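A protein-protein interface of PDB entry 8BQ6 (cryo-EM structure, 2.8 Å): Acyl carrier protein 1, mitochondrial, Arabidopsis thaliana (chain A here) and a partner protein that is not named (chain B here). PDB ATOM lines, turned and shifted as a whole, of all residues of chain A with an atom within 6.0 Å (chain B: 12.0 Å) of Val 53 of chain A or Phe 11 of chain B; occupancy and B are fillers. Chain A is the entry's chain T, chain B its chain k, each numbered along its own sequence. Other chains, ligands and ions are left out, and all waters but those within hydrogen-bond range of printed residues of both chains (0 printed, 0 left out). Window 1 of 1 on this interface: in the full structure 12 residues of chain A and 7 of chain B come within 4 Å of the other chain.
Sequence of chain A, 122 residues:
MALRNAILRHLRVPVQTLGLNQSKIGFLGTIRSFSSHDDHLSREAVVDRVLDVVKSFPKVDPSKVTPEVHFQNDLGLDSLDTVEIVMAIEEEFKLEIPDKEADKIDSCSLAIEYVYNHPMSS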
ATOM      1  N   ASP A  48      26.277 -14.009   5.099  1.00  0.00           N
ATOM      2  CA  ASP A  48      25.972 -12.797   5.848  1.00  0.00           C
ATOM      3  C   ASP A  48      25.438 -11.713   4.921  1.00  0.00           C
ATOM      4  O   ASP A  48      24.442 -11.049   5.229  1.00  0.00           O
ATOM      5  CB  ASP A  48      27.231 -12.333   6.585  1.00  0.00           C
ATOM      6  CG  ASP A  48      27.039 -11.031   7.342  1.00  0.00           C
ATOM      7  OD1 ASP A  48      26.593 -10.022   6.758  1.00  0.00           O
ATOM      8  OD2 ASP A  48      27.344 -11.023   8.552  1.00  0.00           O
ATOM      9  N   ARG A  49      26.083 -11.535   3.765  1.00  0.00           N
ATOM     10  CA  ARG A  49      25.774 -10.396   2.910  1.00  0.00           C
ATOM     11  C   ARG A  49      24.448 -10.559   2.174  1.00  0.00           C
ATOM     12  O   ARG A  49      23.706  -9.582   2.033  1.00  0.00           O
ATOM     13  CB  ARG A  49      26.913 -10.165   1.918  1.00  0.00           C
ATOM     14  CG  ARG A  49      28.139  -9.511   2.538  1.00  0.00           C
ATOM     15  CD  ARG A  49      28.852  -8.640   1.523  1.00  0.00           C
ATOM     16  NE  ARG A  49      30.048  -9.271   0.982  1.00  0.00           N
ATOM     17  CZ  ARG A  49      30.533  -9.034  -0.230  1.00  0.00           C
ATOM     18  NH1 ARG A  49      29.917  -8.221  -1.072  1.00  0.00           N
ATOM     19  NH2 ARG A  49      31.658  -9.632  -0.608  1.00  0.00           N
ATOM     20  N   VAL A  50      24.182 -11.753   1.644  1.00  0.00           N
ATOM     21  CA  VAL A  50      22.929 -11.956   0.858  1.00  0.00           C
ATOM     22  C   VAL A  50      21.731 -11.837   1.809  1.00  0.00           C
ATOM     23  O   VAL A  50      20.750 -11.188   1.429  1.00  0.00           O
ATOM     24  CB  VAL A  50      22.934 -13.286   0.081  1.00  0.00           C
ATOM     25  CG1 VAL A  50      23.223 -14.469   0.979  1.00  0.00           C
ATOM     26  CG2 VAL A  50      21.646 -13.519  -0.685  1.00  0.00           C
ATOM     27  N   LEU A  51      21.827 -12.397   3.016  1.00  0.00           N
ATOM     28  CA  LEU A  51      20.732 -12.269   4.011  1.00  0.00           C
ATOM     29  C   LEU A  51      20.554 -10.787   4.350  1.00  0.00           C
ATOM     30  O   LEU A  51      19.396 -10.355   4.407  1.00  0.00           O
ATOM     31  CB  LEU A  51      21.084 -13.083   5.258  1.00  0.00           C
ATOM     32  CG  LEU A  51      20.409 -14.447   5.382  1.00  0.00           C
ATOM     33  CD1 LEU A  51      21.046 -15.458   4.445  1.00  0.00           C
ATOM     34  CD2 LEU A  51      20.484 -14.943   6.816  1.00  0.00           C
ATOM     35  N   ASP A  52      21.654 -10.045   4.557  1.00  0.00           N
ATOM     36  CA  ASP A  52      21.556  -8.614   4.818  1.00  0.00           C
ATOM     37  C   ASP A  52      20.778  -7.911   3.711  1.00  0.00           C
ATOM     38  O   ASP A  52      20.051  -6.945   3.973  1.00  0.00           O
ATOM     39  CB  ASP A  52      22.955  -8.017   4.962  1.00  0.00           C
ATOM     40  CG  ASP A  52      22.980  -6.788   5.844  1.00  0.00           C
ATOM     41  OD1 ASP A  52      22.178  -5.861   5.605  1.00  0.00           O
ATOM     42  OD2 ASP A  52      23.815  -6.746   6.773  1.00  0.00           O
ATOM     43  N   VAL A  53      20.922  -8.378   2.469  1.00  0.00           N
ATOM     44  CA  VAL A  53      20.192  -7.780   1.351  1.00  0.00           C
ATOM     45  C   VAL A  53      18.695  -8.019   1.503  1.00  0.00           C
ATOM     46  O   VAL A  53      17.877  -7.123   1.256  1.00  0.00           O
ATOM     47  CB  VAL A  53      20.720  -8.324   0.010  1.00  0.00           C
ATOM     48  CG1 VAL A  53      19.756  -7.992  -1.116  1.00  0.00           C
ATOM     49  CG2 VAL A  53      22.096  -7.750  -0.290  1.00  0.00           C
ATOM     50  N   VAL A  54      18.301  -9.211   1.925  1.00  0.00           N
ATOM     51  CA  VAL A  54      16.828  -9.433   1.976  1.00  0.00           C
ATOM     52  C   VAL A  54      16.292  -8.801   3.270  1.00  0.00           C
ATOM     53  O   VAL A  54      15.105  -8.434   3.279  1.00  0.00           O
ATOM     54  CB  VAL A  54      16.446 -10.916   1.793  1.00  0.00           C
ATOM     55  CG1 VAL A  54      16.826 -11.454   0.425  1.00  0.00           C
ATOM     56  CG2 VAL A  54      16.976 -11.811   2.893  1.00  0.00           C
ATOM     57  N   LYS A  55      17.112  -8.625   4.303  1.00  0.00           N
ATOM     58  CA  LYS A  55      16.552  -8.074   5.564  1.00  0.00           C
ATOM     59  C   LYS A  55      16.098  -6.628   5.324  1.00  0.00           C
ATOM     60  O   LYS A  55      15.124  -6.212   5.977  1.00  0.00           O
ATOM     61  CB  LYS A  55      17.570  -8.187   6.702  1.00  0.00           C
ATOM     62  CG  LYS A  55      17.549  -9.524   7.429  1.00  0.00           C
ATOM     63  CD  LYS A  55      18.557  -9.612   8.549  1.00  0.00           C
ATOM     64  CE  LYS A  55      19.526 -10.762   8.377  1.00  0.00           C
ATOM     65  NZ  LYS A  55      20.931 -10.294   8.369  1.00  0.00           N
ATOM     66  N   SER A  56      16.749  -5.914   4.395  1.00  0.00           N
ATOM     67  CA  SER A  56      16.399  -4.523   4.139  1.00  0.00           C
ATOM     68  C   SER A  56      15.055  -4.361   3.444  1.00  0.00           C
ATOM     69  O   SER A  56      14.537  -3.240   3.390  1.00  0.00           O
ATOM     70  CB  SER A  56      17.481  -3.860   3.284  1.00  0.00           C
ATOM     71  OG  SER A  56      18.709  -3.790   3.984  1.00  0.00           O
ATOM     72  N   PHE A  57      14.492  -5.431   2.905  1.00  0.00           N
ATOM     73  CA  PHE A  57      13.242  -5.306   2.175  1.00  0.00           C
ATOM     74  C   PHE A  57      12.128  -4.902   3.133  1.00  0.00           C
ATOM     75  O   PHE A  57      12.002  -5.492   4.212  1.00  0.00           O
ATOM     76  CB  PHE A  57      12.897  -6.608   1.469  1.00  0.00           C
ATOM     77  CG  PHE A  57      12.028  -6.414   0.279  1.00  0.00           C
ATOM     78  CD1 PHE A  57      12.578  -6.097  -0.946  1.00  0.00           C
ATOM     79  CD2 PHE A  57      10.657  -6.509   0.388  1.00  0.00           C
ATOM     80  CE1 PHE A  57      11.778  -5.896  -2.048  1.00  0.00           C
ATOM     81  CE2 PHE A  57       9.853  -6.309  -0.707  1.00  0.00           C
ATOM     82  CZ  PHE A  57      10.413  -6.001  -1.928  1.00  0.00           C
ATOM     83  N   PRO A  58      11.317  -3.897   2.788  1.00  0.00           N
ATOM     84  CA  PRO A  58      10.359  -3.360   3.771  1.00  0.00           C
ATOM     85  C   PRO A  58       9.328  -4.368   4.242  1.00  0.00           C
ATOM     86  O   PRO A  58       9.083  -4.472   5.451  1.00  0.00           O
ATOM     87  CB  PRO A  58       9.704  -2.191   3.021  1.00  0.00           C
ATOM     88  CG  PRO A  58      10.006  -2.428   1.573  1.00  0.00           C
ATOM     89  CD  PRO A  58      11.312  -3.139   1.527  1.00  0.00           C
ATOM     90  N   ASP A  81       8.553  -8.657  -6.239  1.00  0.00           N
ATOM     91  CA  ASP A  81       9.413  -8.353  -5.100  1.00  0.00           C
ATOM     92  C   ASP A  81      10.707  -9.154  -5.157  1.00  0.00           C
ATOM     93  O   ASP A  81      11.762  -8.672  -4.729  1.00  0.00           O
ATOM     94  CB  ASP A  81       8.666  -8.603  -3.797  1.00  0.00           C
ATOM     95  CG  ASP A  81       7.499  -7.664  -3.623  1.00  0.00           C
ATOM     96  OD1 ASP A  81       7.576  -6.757  -2.770  1.00  0.00           O
ATOM     97  OD2 ASP A  81       6.511  -7.819  -4.369  1.00  0.00           O
ATOM     98  N   GLU A  84      13.478  -7.633  -7.609  1.00  0.00           N
ATOM     99  CA  GLU A  84      14.191  -6.500  -7.024  1.00  0.00           C
ATOM    100  C   GLU A  84      15.250  -6.969  -6.040  1.00  0.00           C
ATOM    101  O   GLU A  84      16.325  -6.367  -5.941  1.00  0.00           O
ATOM    102  CB  GLU A  84      13.247  -5.524  -6.325  1.00  0.00           C
ATOM    103  CG  GLU A  84      12.308  -4.757  -7.223  1.00  0.00           C
ATOM    104  CD  GLU A  84      10.869  -5.133  -7.009  1.00  0.00           C
ATOM    105  OE1 GLU A  84       9.973  -4.338  -7.341  1.00  0.00           O
ATOM    106  OE2 GLU A  84      10.636  -6.202  -6.472  1.00  0.00           O
ATOM    107  N   ILE A  85      14.932  -8.021  -5.280  1.00  0.00           N
ATOM    108  CA  ILE A  85      15.938  -8.602  -4.344  1.00  0.00           C
ATOM    109  C   ILE A  85      17.099  -9.137  -5.190  1.00  0.00           C
ATOM    110  O   ILE A  85      18.250  -8.863  -4.827  1.00  0.00           O
ATOM    111  CB  ILE A  85      15.294  -9.683  -3.451  1.00  0.00           C
ATOM    112  CG1 ILE A  85      14.256  -9.085  -2.499  1.00  0.00           C
ATOM    113  CG2 ILE A  85      16.341 -10.477  -2.689  1.00  0.00           C
ATOM    114  CD1 ILE A  85      13.424 -10.115  -1.774  1.00  0.00           C
ATOM    115  N   ALA A  88      19.151  -6.235  -6.189  1.00  0.00           N
ATOM    116  CA  ALA A  88      19.971  -5.736  -5.091  1.00  0.00           C
ATOM    117  C   ALA A  88      21.118  -6.690  -4.789  1.00  0.00           C
ATOM    118  O   ALA A  88      22.220  -6.255  -4.436  1.00  0.00           O
ATOM    119  CB  ALA A  88      19.113  -5.516  -3.847  1.00  0.00           C
ATOM    120  N   ILE A  89      20.873  -7.995  -4.908  1.00  0.00           N
ATOM    121  CA  ILE A  89      21.960  -8.960  -4.781  1.00  0.00           C
ATOM    122  C   ILE A  89      22.953  -8.777  -5.919  1.00  0.00           C
ATOM    123  O   ILE A  89      24.162  -8.977  -5.751  1.00  0.00           O
ATOM    124  CB  ILE A  89      21.395 -10.392  -4.719  1.00  0.00           C
ATOM    125  CG1 ILE A  89      20.760 -10.640  -3.354  1.00  0.00           C
ATOM    126  CG2 ILE A  89      22.476 -11.431  -4.980  1.00  0.00           C
ATOM    127  CD1 ILE A  89      19.773 -11.770  -3.345  1.00  0.00           C
ATOM    128  N   GLU A  92      25.067  -5.817  -5.003  1.00  0.00           N
ATOM    129  CA  GLU A  92      25.851  -6.028  -3.794  1.00  0.00           C
ATOM    130  C   GLU A  92      27.187  -6.685  -4.104  1.00  0.00           C
ATOM    131  O   GLU A  92      28.211  -6.319  -3.516  1.00  0.00           O
ATOM    132  CB  GLU A  92      25.062  -6.870  -2.794  1.00  0.00           C
ATOM    133  CG  GLU A  92      25.886  -7.324  -1.606  1.00  0.00           C
ATOM    134  CD  GLU A  92      26.195  -6.175  -0.665  1.00  0.00           C
ATOM    135  OE1 GLU A  92      25.549  -5.117  -0.795  1.00  0.00           O
ATOM    136  OE2 GLU A  92      27.080  -6.324   0.203  1.00  0.00           O
ATOM    137  N   PHE A  93      27.195  -7.649  -5.020  1.00  0.00           N
ATOM    138  CA  PHE A  93      28.405  -8.336  -5.439  1.00  0.00           C
ATOM    139  C   PHE A  93      28.880  -7.891  -6.814  1.00  0.00           C
ATOM    140  O   PHE A  93      29.823  -8.483  -7.349  1.00  0.00           O
ATOM    141  CB  PHE A  93      28.176  -9.851  -5.437  1.00  0.00           C
ATOM    142  CG  PHE A  93      27.864 -10.417  -4.081  1.00  0.00           C
ATOM    143  CD1 PHE A  93      28.877 -10.693  -3.183  1.00  0.00           C
ATOM    144  CD2 PHE A  93      26.558 -10.684  -3.709  1.00  0.00           C
ATOM    145  CE1 PHE A  93      28.594 -11.215  -1.941  1.00  0.00           C
ATOM    146  CE2 PHE A  93      26.274 -11.204  -2.466  1.00  0.00           C
ATOM    147  CZ  PHE A  93      27.293 -11.469  -1.582  1.00  0.00           C
ATOM    148  N   PRO B   4      11.571   7.448  -3.295  1.00  0.00           N
ATOM    149  CA  PRO B   4      11.598   6.281  -2.400  1.00  0.00           C
ATOM    150  C   PRO B   4      10.263   6.087  -1.664  1.00  0.00           C
ATOM    151  O   PRO B   4      10.257   5.424  -0.640  1.00  0.00           O
ATOM    152  CB  PRO B   4      12.721   6.600  -1.401  1.00  0.00           C
ATOM    153  CG  PRO B   4      12.718   8.104  -1.327  1.00  0.00           C
ATOM    154  CD  PRO B   4      12.357   8.551  -2.728  1.00  0.00           C
ATOM    155  N   LEU B   5       9.176   6.647  -2.206  1.00  0.00           N
ATOM    156  CA  LEU B   5       7.840   6.545  -1.560  1.00  0.00           C
ATOM    157  C   LEU B   5       7.352   5.094  -1.616  1.00  0.00           C
ATOM    158  O   LEU B   5       7.055   4.536  -0.541  1.00  0.00           O
ATOM    159  CB  LEU B   5       6.871   7.476  -2.294  1.00  0.00           C
ATOM    160  CG  LEU B   5       5.553   7.747  -1.571  1.00  0.00           C
ATOM    161  CD1 LEU B   5       5.558   9.130  -0.940  1.00  0.00           C
ATOM    162  CD2 LEU B   5       4.375   7.598  -2.521  1.00  0.00           C
ATOM    163  N   GLY B   6       7.280   4.512  -2.819  1.00  0.00           N
ATOM    164  CA  GLY B   6       6.795   3.126  -2.979  1.00  0.00           C
ATOM    165  C   GLY B   6       7.779   2.096  -2.455  1.00  0.00           C
ATOM    166  O   GLY B   6       8.959   2.445  -2.259  1.00  0.00           O
ATOM    167  N   THR B   7       7.312   0.862  -2.245  1.00  0.00           N
ATOM    168  CA  THR B   7       8.180  -0.210  -1.685  1.00  0.00           C
ATOM    169  C   THR B   7       9.410  -0.418  -2.579  1.00  0.00           C
ATOM    170  O   THR B   7      10.471  -0.759  -2.024  1.00  0.00           O
ATOM    171  CB  THR B   7       7.386  -1.505  -1.470  1.00  0.00           C
ATOM    172  OG1 THR B   7       6.975  -2.015  -2.740  1.00  0.00           O
ATOM    173  CG2 THR B   7       6.177  -1.295  -0.586  1.00  0.00           C
ATOM    174  N   THR B   8       9.275  -0.215  -3.896  1.00  0.00           N
ATOM    175  CA  THR B   8      10.432  -0.337  -4.774  1.00  0.00           C
ATOM    176  C   THR B   8      11.476   0.719  -4.436  1.00  0.00           C
ATOM    177  O   THR B   8      12.660   0.406  -4.262  1.00  0.00           O
ATOM    178  CB  THR B   8       9.997  -0.208  -6.234  1.00  0.00           C
ATOM    179  OG1 THR B   8       8.927  -1.122  -6.491  1.00  0.00           O
ATOM    180  CG2 THR B   8      11.149  -0.556  -7.151  1.00  0.00           C
ATOM    181  N   GLY B   9      11.051   1.979  -4.322  1.00  0.00           N
ATOM    182  CA  GLY B   9      11.981   3.040  -3.980  1.00  0.00           C
ATOM    183  C   GLY B   9      12.547   2.913  -2.580  1.00  0.00           C
ATOM    184  O   GLY B   9      13.722   3.210  -2.354  1.00  0.00           O
ATOM    185  N   GLU B  10      11.725   2.469  -1.623  1.00  0.00           N
ATOM    186  CA  GLU B  10      12.176   2.375  -0.238  1.00  0.00           C
ATOM    187  C   GLU B  10      13.255   1.315  -0.082  1.00  0.00           C
ATOM    188  O   GLU B  10      14.163   1.454   0.747  1.00  0.00           O
ATOM    189  CB  GLU B  10      10.990   2.072   0.679  1.00  0.00           C
ATOM    190  CG  GLU B  10      11.355   1.842   2.139  1.00  0.00           C
ATOM    191  CD  GLU B  10      12.193   2.966   2.718  1.00  0.00           C
ATOM    192  OE1 GLU B  10      11.834   4.144   2.505  1.00  0.00           O
ATOM    193  OE2 GLU B  10      13.201   2.671   3.398  1.00  0.00           O
ATOM    194  N   PHE B  11      13.162   0.240  -0.866  1.00  0.00           N
ATOM    195  CA  PHE B  11      14.184  -0.798  -0.832  1.00  0.00           C
ATOM    196  C   PHE B  11      15.546  -0.245  -1.225  1.00  0.00           C
ATOM    197  O   PHE B  11      16.533  -0.429  -0.504  1.00  0.00           O
ATOM    198  CB  PHE B  11      13.791  -1.929  -1.778  1.00  0.00           C
ATOM    199  CG  PHE B  11      14.655  -3.146  -1.665  1.00  0.00           C
ATOM    200  CD1 PHE B  11      15.545  -3.299  -0.618  1.00  0.00           C
ATOM    201  CD2 PHE B  11      14.624  -4.108  -2.652  1.00  0.00           C
ATOM    202  CE1 PHE B  11      16.347  -4.410  -0.535  1.00  0.00           C
ATOM    203  CE2 PHE B  11      15.427  -5.221  -2.573  1.00  0.00           C
ATOM    204  CZ  PHE B  11      16.290  -5.372  -1.516  1.00  0.00           C
ATOM    205  N   PHE B  12      15.615   0.437  -2.367  1.00  0.00           N
ATOM    206  CA  PHE B  12      16.908   0.814  -2.918  1.00  0.00           C
ATOM    207  C   PHE B  12      17.582   1.901  -2.091  1.00  0.00           C
ATOM    208  O   PHE B  12      18.810   1.894  -1.954  1.00  0.00           O
ATOM    209  CB  PHE B  12      16.729   1.222  -4.378  1.00  0.00           C
ATOM    210  CG  PHE B  12      16.442   0.056  -5.283  1.00  0.00           C
ATOM    211  CD1 PHE B  12      17.236  -1.077  -5.234  1.00  0.00           C
ATOM    212  CD2 PHE B  12      15.358   0.069  -6.143  1.00  0.00           C
ATOM    213  CE1 PHE B  12      16.977  -2.160  -6.047  1.00  0.00           C
ATOM    214  CE2 PHE B  12      15.092  -1.013  -6.957  1.00  0.00           C
ATOM    215  CZ  PHE B  12      15.903  -2.131  -6.907  1.00  0.00           C
ATOM    216  N   ARG B  13      16.809   2.821  -1.509  1.00  0.00           N
ATOM    217  CA  ARG B  13      17.407   3.771  -0.576  1.00  0.00           C
ATOM    218  C   ARG B  13      17.930   3.072   0.669  1.00  0.00           C
ATOM    219  O   ARG B  13      18.959   3.473   1.225  1.00  0.00           O
ATOM    220  CB  ARG B  13      16.412   4.855  -0.180  1.00  0.00           C
ATOM    221  CG  ARG B  13      17.090   6.186   0.051  1.00  0.00           C
ATOM    222  CD  ARG B  13      16.346   7.021   1.061  1.00  0.00           C
ATOM    223  NE  ARG B  13      16.964   6.972   2.381  1.00  0.00           N
ATOM    224  CZ  ARG B  13      16.309   6.706   3.503  1.00  0.00           C
ATOM    225  NH1 ARG B  13      15.013   6.436   3.499  1.00  0.00           N
ATOM    226  NH2 ARG B  13      16.969   6.714   4.657  1.00  0.00           N
ATOM    227  N   ARG B  14      17.222   2.047   1.139  1.00  0.00           N
ATOM    228  CA  ARG B  14      17.708   1.297   2.288  1.00  0.00           C
ATOM    229  C   ARG B  14      19.030   0.609   1.974  1.00  0.00           C
ATOM    230  O   ARG B  14      19.926   0.555   2.821  1.00  0.00           O
ATOM    231  CB  ARG B  14      16.666   0.276   2.732  1.00  0.00           C
ATOM    232  CG  ARG B  14      16.669   0.049   4.221  1.00  0.00           C
ATOM    233  CD  ARG B  14      15.772   1.052   4.930  1.00  0.00           C
ATOM    234  NE  ARG B  14      14.366   0.867   4.588  1.00  0.00           N
ATOM    235  CZ  ARG B  14      13.649  -0.203   4.905  1.00  0.00           C
ATOM    236  NH1 ARG B  14      14.176  -1.219   5.570  1.00  0.00           N
ATOM    237  NH2 ARG B  14      12.369  -0.255   4.549  1.00  0.00           N
ATOM    238  N   ARG B  15      19.168   0.073   0.761  1.00  0.00           N
ATOM    239  CA  ARG B  15      20.422  -0.557   0.366  1.00  0.00           C
ATOM    240  C   ARG B  15      21.518   0.452   0.057  1.00  0.00           C
ATOM    241  O   ARG B  15      22.699   0.093   0.093  1.00  0.00           O
ATOM    242  CB  ARG B  15      20.198  -1.448  -0.847  1.00  0.00           C
ATOM    243  CG  ARG B  15      19.197  -2.549  -0.614  1.00  0.00           C
ATOM    244  CD  ARG B  15      19.703  -3.564   0.402  1.00  0.00           C
ATOM    245  NE  ARG B  15      21.114  -3.883   0.223  1.00  0.00           N
ATOM    246  CZ  ARG B  15      21.925  -4.271   1.198  1.00  0.00           C
ATOM    247  NH1 ARG B  15      21.480  -4.475   2.428  1.00  0.00           N
ATOM    248  NH2 ARG B  15      23.213  -4.469   0.933  1.00  0.00           N
ATOM    249  N   ASP B  16      21.156   1.693  -0.269  1.00  0.00           N
ATOM    250  CA  ASP B  16      22.113   2.747  -0.569  1.00  0.00           C
ATOM    251  C   ASP B  16      22.568   3.472   0.676  1.00  0.00           C
ATOM    252  O   ASP B  16      23.142   4.565   0.586  1.00  0.00           O
ATOM    253  CB  ASP B  16      21.502   3.743  -1.547  1.00  0.00           C
ATOM    254  CG  ASP B  16      21.575   3.263  -2.965  1.00  0.00           C
ATOM    255  OD1 ASP B  16      22.651   2.773  -3.360  1.00  0.00           O
ATOM    256  OD2 ASP B  16      20.557   3.357  -3.679  1.00  0.00           O
ATOM    257  N   GLU B  17      22.312   2.886   1.837  1.00  0.00           N
ATOM    258  CA  GLU B  17      22.529   3.600   3.084  1.00  0.00           C
ATOM    259  C   GLU B  17      24.012   3.683   3.426  1.00  0.00           C
ATOM    260  O   GLU B  17      24.401   4.497   4.271  1.00  0.00           O
ATOM    261  CB  GLU B  17      21.657   2.940   4.166  1.00  0.00           C
ATOM    262  CG  GLU B  17      20.161   3.091   3.986  1.00  0.00           C
ATOM    263  CD  GLU B  17      19.386   2.381   5.010  1.00  0.00           C
ATOM    264  OE1 GLU B  17      20.012   1.611   5.756  1.00  0.00           O
ATOM    265  OE2 GLU B  17      18.139   2.555   5.030  1.00  0.00           O
ATOM    266  N   TRP B  18      24.857   2.885   2.762  1.00  0.00           N
ATOM    267  CA  TRP B  18      26.301   3.067   2.893  1.00  0.00           C
ATOM    268  C   TRP B  18      26.811   4.269   2.103  1.00  0.00           C
ATOM    269  O   TRP B  18      27.922   4.740   2.367  1.00  0.00           O
ATOM    270  CB  TRP B  18      27.065   1.814   2.443  1.00  0.00           C
ATOM    271  CG  TRP B  18      26.960   1.510   0.973  1.00  0.00           C
ATOM    272  CD1 TRP B  18      26.074   0.665   0.370  1.00  0.00           C
ATOM    273  CD2 TRP B  18      27.764   2.059  -0.078  1.00  0.00           C
ATOM    274  NE1 TRP B  18      26.278   0.652  -0.987  1.00  0.00           N
ATOM    275  CE2 TRP B  18      27.310   1.499  -1.287  1.00  0.00           C
ATOM    276  CE3 TRP B  18      28.825   2.967  -0.113  1.00  0.00           C
ATOM    277  CZ2 TRP B  18      27.879   1.820  -2.515  1.00  0.00           C
ATOM    278  CZ3 TRP B  18      29.385   3.284  -1.331  1.00  0.00           C
ATOM    279  CH2 TRP B  18      28.914   2.713  -2.515  1.00  0.00           C
ATOM    280  N   ARG B  19      26.036   4.777   1.140  1.00  0.00           N
ATOM    281  CA  ARG B  19      26.498   5.902   0.330  1.00  0.00           C
ATOM    282  C   ARG B  19      26.554   7.210   1.106  1.00  0.00           C
ATOM    283  O   ARG B  19      26.974   8.227   0.543  1.00  0.00           O
ATOM    284  CB  ARG B  19      25.611   6.068  -0.903  1.00  0.00           C
ATOM    285  CG  ARG B  19      25.986   5.127  -2.031  1.00  0.00           C
ATOM    286  CD  ARG B  19      24.978   5.151  -3.153  1.00  0.00           C
ATOM    287  NE  ARG B  19      24.743   3.812  -3.676  1.00  0.00           N
ATOM    288  CZ  ARG B  19      25.444   3.260  -4.656  1.00  0.00           C
ATOM    289  NH1 ARG B  19      26.460   3.894  -5.220  1.00  0.00           N
ATOM    290  NH2 ARG B  19      25.123   2.042  -5.076  1.00  0.00           N
ATOM    291  N   LYS B  20      26.143   7.212   2.372  1.00  0.00           N
ATOM    292  CA  LYS B  20      26.333   8.351   3.259  1.00  0.00           C
ATOM    293  C   LYS B  20      27.691   8.332   3.936  1.00  0.00           C
ATOM    294  O   LYS B  20      27.848   8.923   5.011  1.00  0.00           O
ATOM    295  CB  LYS B  20      25.222   8.395   4.310  1.00  0.00           C
ATOM    296  CG  LYS B  20      23.822   8.344   3.729  1.00  0.00           C
ATOM    297  CD  LYS B  20      23.692   9.281   2.536  1.00  0.00           C
ATOM    298  CE  LYS B  20      22.249   9.416   2.093  1.00  0.00           C
ATOM    299  NZ  LYS B  20      21.874  10.843   1.889  1.00  0.00           N
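Of the 18 printed residues of chain A, 9 touch a printed residue of chain B.
Hydrophobic or aromatic side chains of chain A within 4 Å of the printed part of chain B: Val 53, Phe 57, Pro 58 and Ala 88.
Of the 17 printed residues of chain B, 5 touch a printed residue of chain A.
Among the printed residues, 13 pairs touch across the chains.
Among the printed residues, Asp or Glu carboxylates within 4 Å of a Lys or Arg side-chain nitrogen of the other chain: Asp 52 of chain A with Arg 15 of chain B (3.5 Å) and Glu 92 of chain A with Arg 15 of chain B (3.0 Å).
The side-chain carboxylate (OE2) of Glu 92 of chain A is in salt-bridge range of the guanidinium group (NH1) of Arg 49 of chain A (3.6 Å).
The side-chain hydroxyl (OG) of Ser 56 of chain A sits at hydrogen-bond distance from the backbone carbonyl oxygen (O) of Asp 52 of chain A, 3.4 Å away.
The side-chain carboxylate (OE2) of Glu 84 of chain A sits close to the backbone NH (N) of Asp 81 of chain A, 3.2 Å away.
The guanidinium group of Arg 14 of chain B lies within salt-bridge range of the side-chain carboxylate of Glu 10 of chain B, 2.5 Å away.
Phe 11 of chain B touches Val 53 of chain A.
Arg 15 of chain B touches Val 53 of chain A.
Phe 57 of chain A touches Phe 11 of chain B.
Pro 58 of chain A touches Thr 7 of chain B.
Pro 58 of chain A touches Arg 14 of chain B.
Glu 84 of chain A touches Phe 11 of chain B.
Ile 85 of chain A touches Phe 11 of chain B.
Ala 88 of chain A touches Phe 11 of chain B.
No residue of chain B comes within 4 Å of Val 50 of chain A.
No residue of chain B comes within 4 Å of Leu 51 of chain A.
Asp 52 of chain A touches one residue of chain B.
Val 53 of chain A touches just these residues of chain B: Phe 11 (3.6 Å) and Arg 15 (3.7 Å).
No residue of chain B comes within 4 Å of Val 54 of chain A.
Printed residues of chain B within 4 Å of Pro 58 of chain A: Thr 7 and Arg 14.
Glu 84 of chain A touches just these residues of chain B: Thr 8 and Phe 11.
Ile 85 of chain A touches one residue of chain B.
Of chain B, only Phe 11 (3.7 Å) comes within 4 Å of Ala 88 of chain A.
Glu 92 of chain A touches just one residue of chain B: Arg 15 (3.0 Å).
Of the printed residues of chain A, Thr 7 of chain B touches Pro 58 (3.99 Å).
Of the printed residues of chain A, Thr 8 of chain B touches Glu 84.
Of chain A, only Val 53, Phe 57, Glu 84, Ile 85 and Ala 88 come within 4 Å of Phe 11 of chain B.
Of the printed residues of chain A, Arg 14 of chain B touches Ser 56 and Pro 58.
Printed residues of chain A within 4 Å of Arg 15 of chain B: Asp 52 (3.2 Å), Val 53 (3.7 Å), Ser 56 (3.3 Å) and Glu 92 (3.0 Å).
The nearest residue of chain B that does not touch Val 53 of chain A is Arg 14 of chain B (7.6 Å).
The nearest residue of chain A that does not touch Phe 11 of chain B is Ser 56 of chain A (4.02 Å).
The side-chain carboxylate of Asp 52 of chain A is in salt-bridge range of the guanidinium group of Arg 15 of chain B (3.5 Å).
The backbone carbonyl oxygen of Ser 56 of chain A lies within hydrogen-bond range of the guanidinium group of Arg 14 of chain B (3.0 Å).
The side-chain hydroxyl (OG) of Ser 56 of chain A is in hydrogen-bond range of the guanidinium group (NH1) of Arg 15 of chain B (3.3 Å).
The side-chain hydroxyl (OG1) of Thr 8 of chain B is in hydrogen-bond range of the side-chain carboxylate (OE1) of Glu 84 of chain A (3.5 Å).
NH2 of Arg 15 of chain B lies within salt-bridge range of OE1 of Glu 92 of chain A (3.0 Å).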
